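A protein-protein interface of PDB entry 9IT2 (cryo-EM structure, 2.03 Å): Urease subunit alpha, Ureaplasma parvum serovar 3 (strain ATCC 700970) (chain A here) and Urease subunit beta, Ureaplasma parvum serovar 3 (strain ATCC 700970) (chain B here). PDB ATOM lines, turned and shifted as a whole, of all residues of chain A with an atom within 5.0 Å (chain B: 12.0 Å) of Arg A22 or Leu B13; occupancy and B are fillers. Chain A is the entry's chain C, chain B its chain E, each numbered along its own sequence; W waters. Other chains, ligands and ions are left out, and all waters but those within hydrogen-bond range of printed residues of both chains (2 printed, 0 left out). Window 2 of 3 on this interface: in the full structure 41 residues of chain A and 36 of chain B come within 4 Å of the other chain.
The backbone NH (N) of Arg A22 lies within hydrogen-bond range of the backbone carbonyl oxygen (O) of Ala B17. The backbone carbonyl oxygen (O) of Val B14 lies within hydrogen-bond range of the guanidinium group (NE) of Arg A22, 3.4 Å away. The backbone NH of Asn B19 sits at hydrogen-bond distance from the backbone carbonyl oxygen of Ser A20 (2.6 Å). The backbone NH of Gly B16 is in hydrogen-bond range of the backbone carbonyl oxygen of Gly A24, at 3.0 Å.
The backbone carbonyl oxygen (O) of Pro A443 sits at hydrogen-bond distance from the backbone NH (N) of Gly A24, 2.8 Å away. The guanidinium group (NH1) of Arg A22 lies within hydrogen-bond range of the backbone carbonyl oxygen (O) of Thr A26. OD2 of Asp A25 lies within salt-bridge range of NE of Arg A594, at 2.9 Å.
Ser A20 touches Ile B18. Val A21 touches Gly B16 (CG2 to O, 3.98 Å). Val A21 touches Ala B17. Leu B13 touches Arg A22 (CD1 to CZ, 3.8 Å). O of Arg A22 touches CA of Gly B16, 3.2 Å away. Gly A24 touches Pro B15 (O to CA, 3.2 Å). Trp A29 touches Ala B17. Asn B19 touches Trp A29 (N to CZ3, 3.7 Å). CA of Gly B16 touches C of Pro A443, at 3.8 Å. Leu B13 touches Arg A594.
Of chain B, only Ala B17 (3.96 Å), Ile B18 (3.3 Å) and Asn B19 (2.6 Å) come within 4 Å of Ser A20. Printed residues of chain B within 4 Å of Val A21: Gly B16 and Ala B17. Arg A22 touches just these residues of chain B: Leu B13 (3.8 Å), Val B14 (3.4 Å), Gly B16 (3.2 Å) and Ala B17 (2.8 Å). Gly A24 touches two residues of chain B. No residue of chain B comes within 4 Å of Thr A26. Of chain B, only Ala B17 (3.4 Å) and Asn B19 (3.7 Å) come within 4 Å of Trp A29. Pro A443 touches one residue of chain B. Of the printed residues of chain A, Leu B13 touches Arg A22 (3.8 Å) and Arg A594 (3.7 Å). Printed residues of chain A within 4 Å of Pro B15: Gly A24 (3.2 Å). Printed residues of chain A within 4 Å of Gly B16: Val A21, Arg A22, Gly A24 and Pro A443. Printed residues of chain A within 4 Å of Ile B18: Ser A20. Of the printed residues of chain A, Asn B19 touches Ser A20 (2.6 Å) and Trp A29 (3.7 Å). Phe B20 touches none of the printed residues of chain A. The nearest residue of chain A that does not touch Leu B13 is Asp A25 (4.2 Å). The nearest printed residue of chain A that does not touch Pro B15 is Asp A25 (4.2 Å).
Hydrophobic or aromatic side chains of chain A within 4 Å of the printed part of chain B: Val A21, Trp A29 and Pro A443. Hydrophobic or aromatic side chains of chain B within 4 Å of the printed part of chain A: Leu B13, Pro B15, Ala B17 and Ile B18. Among the printed residues, 15 pairs touch across the chains. Among the printed residues, no Asp or Glu carboxylate lies within 4 Å of a Lys or Arg side-chain nitrogen of the other chain.
Water W2 lies within hydrogen-bond range of the guanidinium group of Arg A22 (2.7 Å) and the backbone NH of Val B14 (3.1 Å). Water W1 lies within hydrogen-bond range of OG of Ser A20 and OD1 of Asn B19.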
ATOM      1  N   SER A  20       4.848  21.531   6.997  1.00  0.00           N
ATOM      2  CA  SER A  20       5.003  22.667   7.890  1.00  0.00           C
ATOM      3  C   SER A  20       6.401  22.667   8.487  1.00  0.00           C
ATOM      4  O   SER A  20       6.990  21.612   8.731  1.00  0.00           O
ATOM      5  CB  SER A  20       3.959  22.647   9.016  1.00  0.00           C
ATOM      6  OG  SER A  20       2.657  22.861   8.505  1.00  0.00           O
ATOM      7  N   VAL A  21       6.928  23.866   8.717  1.00  0.00           N
ATOM      8  CA  VAL A  21       8.238  24.038   9.332  1.00  0.00           C
ATOM      9  C   VAL A  21       8.122  25.040  10.473  1.00  0.00           C
ATOM     10  O   VAL A  21       7.350  26.004  10.397  1.00  0.00           O
ATOM     11  CB  VAL A  21       9.309  24.470   8.301  1.00  0.00           C
ATOM     12  CG1 VAL A  21       9.020  25.846   7.740  1.00  0.00           C
ATOM     13  CG2 VAL A  21      10.703  24.414   8.915  1.00  0.00           C
ATOM     14  N   ARG A  22       8.868  24.785  11.547  1.00  0.00           N
ATOM     15  CA  ARG A  22       8.848  25.619  12.742  1.00  0.00           C
ATOM     16  C   ARG A  22       9.821  26.780  12.585  1.00  0.00           C
ATOM     17  O   ARG A  22      10.972  26.584  12.185  1.00  0.00           O
ATOM     18  CB  ARG A  22       9.210  24.790  13.975  1.00  0.00           C
ATOM     19  CG  ARG A  22       9.265  25.580  15.272  1.00  0.00           C
ATOM     20  CD  ARG A  22      10.065  24.844  16.334  1.00  0.00           C
ATOM     21  NE  ARG A  22       9.403  23.621  16.772  1.00  0.00           N
ATOM     22  CZ  ARG A  22       8.424  23.577  17.666  1.00  0.00           C
ATOM     23  NH1 ARG A  22       7.961  24.676  18.238  1.00  0.00           N
ATOM     24  NH2 ARG A  22       7.897  22.401  17.993  1.00  0.00           N
ATOM     25  N   LEU A  23       9.356  27.985  12.901  1.00  0.00           N
ATOM     26  CA  LEU A  23      10.191  29.181  12.820  1.00  0.00           C
ATOM     27  C   LEU A  23      11.127  29.210  14.022  1.00  0.00           C
ATOM     28  O   LEU A  23      10.710  29.513  15.141  1.00  0.00           O
ATOM     29  CB  LEU A  23       9.325  30.434  12.761  1.00  0.00           C
ATOM     30  CG  LEU A  23       8.326  30.518  11.606  1.00  0.00           C
ATOM     31  CD1 LEU A  23       7.595  31.850  11.626  1.00  0.00           C
ATOM     32  CD2 LEU A  23       9.032  30.310  10.275  1.00  0.00           C
ATOM     33  N   GLY A  24      12.401  28.900  13.786  1.00  0.00           N
ATOM     34  CA  GLY A  24      13.393  28.930  14.849  1.00  0.00           C
ATOM     35  C   GLY A  24      13.026  28.007  15.992  1.00  0.00           C
ATOM     36  O   GLY A  24      12.564  26.878  15.792  1.00  0.00           O
ATOM     37  N   ASP A  25      13.222  28.496  17.216  1.00  0.00           N
ATOM     38  CA  ASP A  25      12.831  27.781  18.421  1.00  0.00           C
ATOM     39  C   ASP A  25      11.548  28.336  19.032  1.00  0.00           C
ATOM     40  O   ASP A  25      11.279  28.102  20.214  1.00  0.00           O
ATOM     41  CB  ASP A  25      13.965  27.809  19.448  1.00  0.00           C
ATOM     42  CG  ASP A  25      14.221  29.198  19.998  1.00  0.00           C
ATOM     43  OD1 ASP A  25      13.996  30.182  19.263  1.00  0.00           O
ATOM     44  OD2 ASP A  25      14.650  29.307  21.165  1.00  0.00           O
ATOM     45  N   THR A  26      10.758  29.070  18.251  1.00  0.00           N
ATOM     46  CA  THR A  26       9.483  29.590  18.714  1.00  0.00           C
ATOM     47  C   THR A  26       8.413  28.501  18.646  1.00  0.00           C
ATOM     48  O   THR A  26       8.666  27.364  18.237  1.00  0.00           O
ATOM     49  CB  THR A  26       9.063  30.803  17.884  1.00  0.00           C
ATOM     50  OG1 THR A  26       8.627  30.369  16.589  1.00  0.00           O
ATOM     51  CG2 THR A  26      10.220  31.775  17.719  1.00  0.00           C
ATOM     52  N   ASN A  27       7.196  28.859  19.045  1.00  0.00           N
ATOM     53  CA  ASN A  27       6.045  27.972  18.956  1.00  0.00           C
ATOM     54  C   ASN A  27       5.275  28.138  17.652  1.00  0.00           C
ATOM     55  O   ASN A  27       4.149  27.644  17.543  1.00  0.00           O
ATOM     56  CB  ASN A  27       5.107  28.200  20.148  1.00  0.00           C
ATOM     57  CG  ASN A  27       4.713  29.660  20.319  1.00  0.00           C
ATOM     58  OD1 ASN A  27       4.740  30.444  19.371  1.00  0.00           O
ATOM     59  ND2 ASN A  27       4.345  30.029  21.541  1.00  0.00           N
ATOM     60  N   LEU A  28       5.852  28.821  16.668  1.00  0.00           N
ATOM     61  CA  LEU A  28       5.162  29.157  15.432  1.00  0.00           C
ATOM     62  C   LEU A  28       5.516  28.173  14.324  1.00  0.00           C
ATOM     63  O   LEU A  28       6.674  27.768  14.183  1.00  0.00           O
ATOM     64  CB  LEU A  28       5.509  30.581  14.994  1.00  0.00           C
ATOM     65  CG  LEU A  28       5.264  31.665  16.045  1.00  0.00           C
ATOM     66  CD1 LEU A  28       6.011  32.943  15.693  1.00  0.00           C
ATOM     67  CD2 LEU A  28       3.772  31.931  16.201  1.00  0.00           C
ATOM     68  N   TRP A  29       4.507  27.794  13.544  1.00  0.00           N
ATOM     69  CA  TRP A  29       4.657  26.921  12.389  1.00  0.00           C
ATOM     70  C   TRP A  29       4.140  27.633  11.147  1.00  0.00           C
ATOM     71  O   TRP A  29       3.137  28.350  11.208  1.00  0.00           O
ATOM     72  CB  TRP A  29       3.881  25.610  12.569  1.00  0.00           C
ATOM     73  CG  TRP A  29       4.424  24.686  13.610  1.00  0.00           C
ATOM     74  CD1 TRP A  29       4.159  24.709  14.948  1.00  0.00           C
ATOM     75  CD2 TRP A  29       5.294  23.569  13.392  1.00  0.00           C
ATOM     76  NE1 TRP A  29       4.827  23.689  15.581  1.00  0.00           N
ATOM     77  CE2 TRP A  29       5.530  22.974  14.648  1.00  0.00           C
ATOM     78  CE3 TRP A  29       5.906  23.022  12.261  1.00  0.00           C
ATOM     79  CZ2 TRP A  29       6.351  21.859  14.802  1.00  0.00           C
ATOM     80  CZ3 TRP A  29       6.720  21.915  12.416  1.00  0.00           C
ATOM     81  CH2 TRP A  29       6.934  21.345  13.677  1.00  0.00           C
ATOM     82  N   PRO A 443      15.814  27.516   8.720  1.00  0.00           N
ATOM     83  CA  PRO A 443      14.636  27.514   9.608  1.00  0.00           C
ATOM     84  C   PRO A 443      14.974  27.436  11.087  1.00  0.00           C
ATOM     85  O   PRO A 443      14.287  28.061  11.904  1.00  0.00           O
ATOM     86  CB  PRO A 443      13.860  26.280   9.136  1.00  0.00           C
ATOM     87  CG  PRO A 443      14.221  26.150   7.699  1.00  0.00           C
ATOM     88  CD  PRO A 443      15.664  26.569   7.602  1.00  0.00           C
ATOM     89  N   ARG A 594      19.533  30.756  23.597  1.00  0.00           N
ATOM     90  CA  ARG A 594      19.868  29.567  22.819  1.00  0.00           C
ATOM     91  C   ARG A 594      20.714  29.885  21.592  1.00  0.00           C
ATOM     92  O   ARG A 594      21.295  28.964  21.006  1.00  0.00           O
ATOM     93  CB  ARG A 594      18.592  28.839  22.383  1.00  0.00           C
ATOM     94  CG  ARG A 594      18.804  27.371  22.025  1.00  0.00           C
ATOM     95  CD  ARG A 594      17.549  26.735  21.435  1.00  0.00           C
ATOM     96  NE  ARG A 594      16.333  27.166  22.114  1.00  0.00           N
ATOM     97  CZ  ARG A 594      15.856  26.614  23.220  1.00  0.00           C
ATOM     98  NH1 ARG A 594      16.457  25.583  23.793  1.00  0.00           N
ATOM     99  NH2 ARG A 594      14.747  27.104  23.764  1.00  0.00           N
ATOM    100  N   GLY B  11       6.724  17.132  22.966  1.00  0.00           N
ATOM    101  CA  GLY B  11       7.955  16.367  22.903  1.00  0.00           C
ATOM    102  C   GLY B  11       9.199  17.233  22.931  1.00  0.00           C
ATOM    103  O   GLY B  11       9.157  18.379  23.376  1.00  0.00           O
ATOM    104  N   LYS B  12      10.312  16.676  22.459  1.00  0.00           N
ATOM    105  CA  LYS B  12      11.565  17.418  22.417  1.00  0.00           C
ATOM    106  C   LYS B  12      11.449  18.607  21.472  1.00  0.00           C
ATOM    107  O   LYS B  12      10.956  18.477  20.347  1.00  0.00           O
ATOM    108  CB  LYS B  12      12.704  16.498  21.977  1.00  0.00           C
ATOM    109  CG  LYS B  12      14.005  17.218  21.668  1.00  0.00           C
ATOM    110  CD  LYS B  12      15.102  16.237  21.292  1.00  0.00           C
ATOM    111  CE  LYS B  12      16.369  16.962  20.874  1.00  0.00           C
ATOM    112  NZ  LYS B  12      17.552  16.059  20.869  1.00  0.00           N
ATOM    113  N   LEU B  13      11.908  19.769  21.930  1.00  0.00           N
ATOM    114  CA  LEU B  13      11.872  20.983  21.121  1.00  0.00           C
ATOM    115  C   LEU B  13      13.026  20.949  20.126  1.00  0.00           C
ATOM    116  O   LEU B  13      14.193  21.063  20.514  1.00  0.00           O
ATOM    117  CB  LEU B  13      11.947  22.222  22.007  1.00  0.00           C
ATOM    118  CG  LEU B  13      12.174  23.547  21.277  1.00  0.00           C
ATOM    119  CD1 LEU B  13      10.976  23.890  20.405  1.00  0.00           C
ATOM    120  CD2 LEU B  13      12.464  24.668  22.264  1.00  0.00           C
ATOM    121  N   VAL B  14      12.705  20.793  18.848  1.00  0.00           N
ATOM    122  CA  VAL B  14      13.689  20.785  17.773  1.00  0.00           C
ATOM    123  C   VAL B  14      13.520  22.081  16.981  1.00  0.00           C
ATOM    124  O   VAL B  14      12.513  22.247  16.277  1.00  0.00           O
ATOM    125  CB  VAL B  14      13.536  19.554  16.870  1.00  0.00           C
ATOM    126  CG1 VAL B  14      14.478  19.650  15.680  1.00  0.00           C
ATOM    127  CG2 VAL B  14      13.796  18.282  17.660  1.00  0.00           C
ATOM    128  N   PRO B  15      14.454  23.026  17.077  1.00  0.00           N
ATOM    129  CA  PRO B  15      14.344  24.253  16.278  1.00  0.00           C
ATOM    130  C   PRO B  15      14.340  23.945  14.788  1.00  0.00           C
ATOM    131  O   PRO B  15      15.097  23.099  14.307  1.00  0.00           O
ATOM    132  CB  PRO B  15      15.584  25.059  16.682  1.00  0.00           C
ATOM    133  CG  PRO B  15      16.044  24.467  17.971  1.00  0.00           C
ATOM    134  CD  PRO B  15      15.636  23.029  17.954  1.00  0.00           C
ATOM    135  N   GLY B  16      13.481  24.651  14.058  1.00  0.00           N
ATOM    136  CA  GLY B  16      13.344  24.409  12.633  1.00  0.00           C
ATOM    137  C   GLY B  16      12.854  23.022  12.289  1.00  0.00           C
ATOM    138  O   GLY B  16      13.255  22.467  11.260  1.00  0.00           O
ATOM    139  N   ALA B  17      11.999  22.441  13.125  1.00  0.00           N
ATOM    140  CA  ALA B  17      11.476  21.110  12.861  1.00  0.00           C
ATOM    141  C   ALA B  17      10.518  21.136  11.674  1.00  0.00           C
ATOM    142  O   ALA B  17       9.925  22.164  11.338  1.00  0.00           O
ATOM    143  CB  ALA B  17      10.766  20.554  14.095  1.00  0.00           C
ATOM    144  N   ILE B  18      10.369  19.979  11.037  1.00  0.00           N
ATOM    145  CA  ILE B  18       9.517  19.822   9.865  1.00  0.00           C
ATOM    146  C   ILE B  18       8.378  18.875  10.213  1.00  0.00           C
ATOM    147  O   ILE B  18       8.606  17.798  10.778  1.00  0.00           O
ATOM    148  CB  ILE B  18      10.312  19.303   8.655  1.00  0.00           C
ATOM    149  CG1 ILE B  18      11.243  20.395   8.124  1.00  0.00           C
ATOM    150  CG2 ILE B  18       9.368  18.829   7.563  1.00  0.00           C
ATOM    151  CD1 ILE B  18      12.406  19.867   7.319  1.00  0.00           C
ATOM    152  N   ASN B  19       7.154  19.280   9.885  1.00  0.00           N
ATOM    153  CA  ASN B  19       5.977  18.430  10.002  1.00  0.00           C
ATOM    154  C   ASN B  19       5.483  18.103   8.599  1.00  0.00           C
ATOM    155  O   ASN B  19       5.224  19.010   7.802  1.00  0.00           O
ATOM    156  CB  ASN B  19       4.880  19.115  10.818  1.00  0.00           C
ATOM    157  CG  ASN B  19       3.748  18.175  11.174  1.00  0.00           C
ATOM    158  OD1 ASN B  19       2.677  18.216  10.567  1.00  0.00           O
ATOM    159  ND2 ASN B  19       3.979  17.320  12.162  1.00  0.00           N
ATOM    160  N   PHE B  20       5.352  16.815   8.302  1.00  0.00           N
ATOM    161  CA  PHE B  20       4.986  16.368   6.966  1.00  0.00           C
ATOM    162  C   PHE B  20       3.486  16.127   6.859  1.00  0.00           C
ATOM    163  O   PHE B  20       2.825  15.736   7.824  1.00  0.00           O
ATOM    164  CB  PHE B  20       5.737  15.089   6.599  1.00  0.00           C
ATOM    165  CG  PHE B  20       7.200  15.297   6.356  1.00  0.00           C
ATOM    166  CD1 PHE B  20       7.637  16.058   5.287  1.00  0.00           C
ATOM    167  CD2 PHE B  20       8.141  14.734   7.202  1.00  0.00           C
ATOM    168  CE1 PHE B  20       8.981  16.251   5.062  1.00  0.00           C
ATOM    169  CE2 PHE B  20       9.488  14.924   6.983  1.00  0.00           C
ATOM    170  CZ  PHE B  20       9.911  15.684   5.911  1.00  0.00           C
ATOM    171  N   ALA B  21       2.956  16.366   5.663  1.00  0.00           N
ATOM    172  CA  ALA B  21       1.568  16.062   5.367  1.00  0.00           C
ATOM    173  C   ALA B  21       1.403  14.569   5.083  1.00  0.00           C
ATOM    174  O   ALA B  21       2.374  13.816   4.980  1.00  0.00           O
ATOM    175  CB  ALA B  21       1.078  16.892   4.180  1.00  0.00           C
HETATM  176  O   HOH W   1       1.496  20.272   8.084  1.00  0.00           O
HETATM  177  O   HOH W   2       9.989  20.764  17.382  1.00  0.00           O
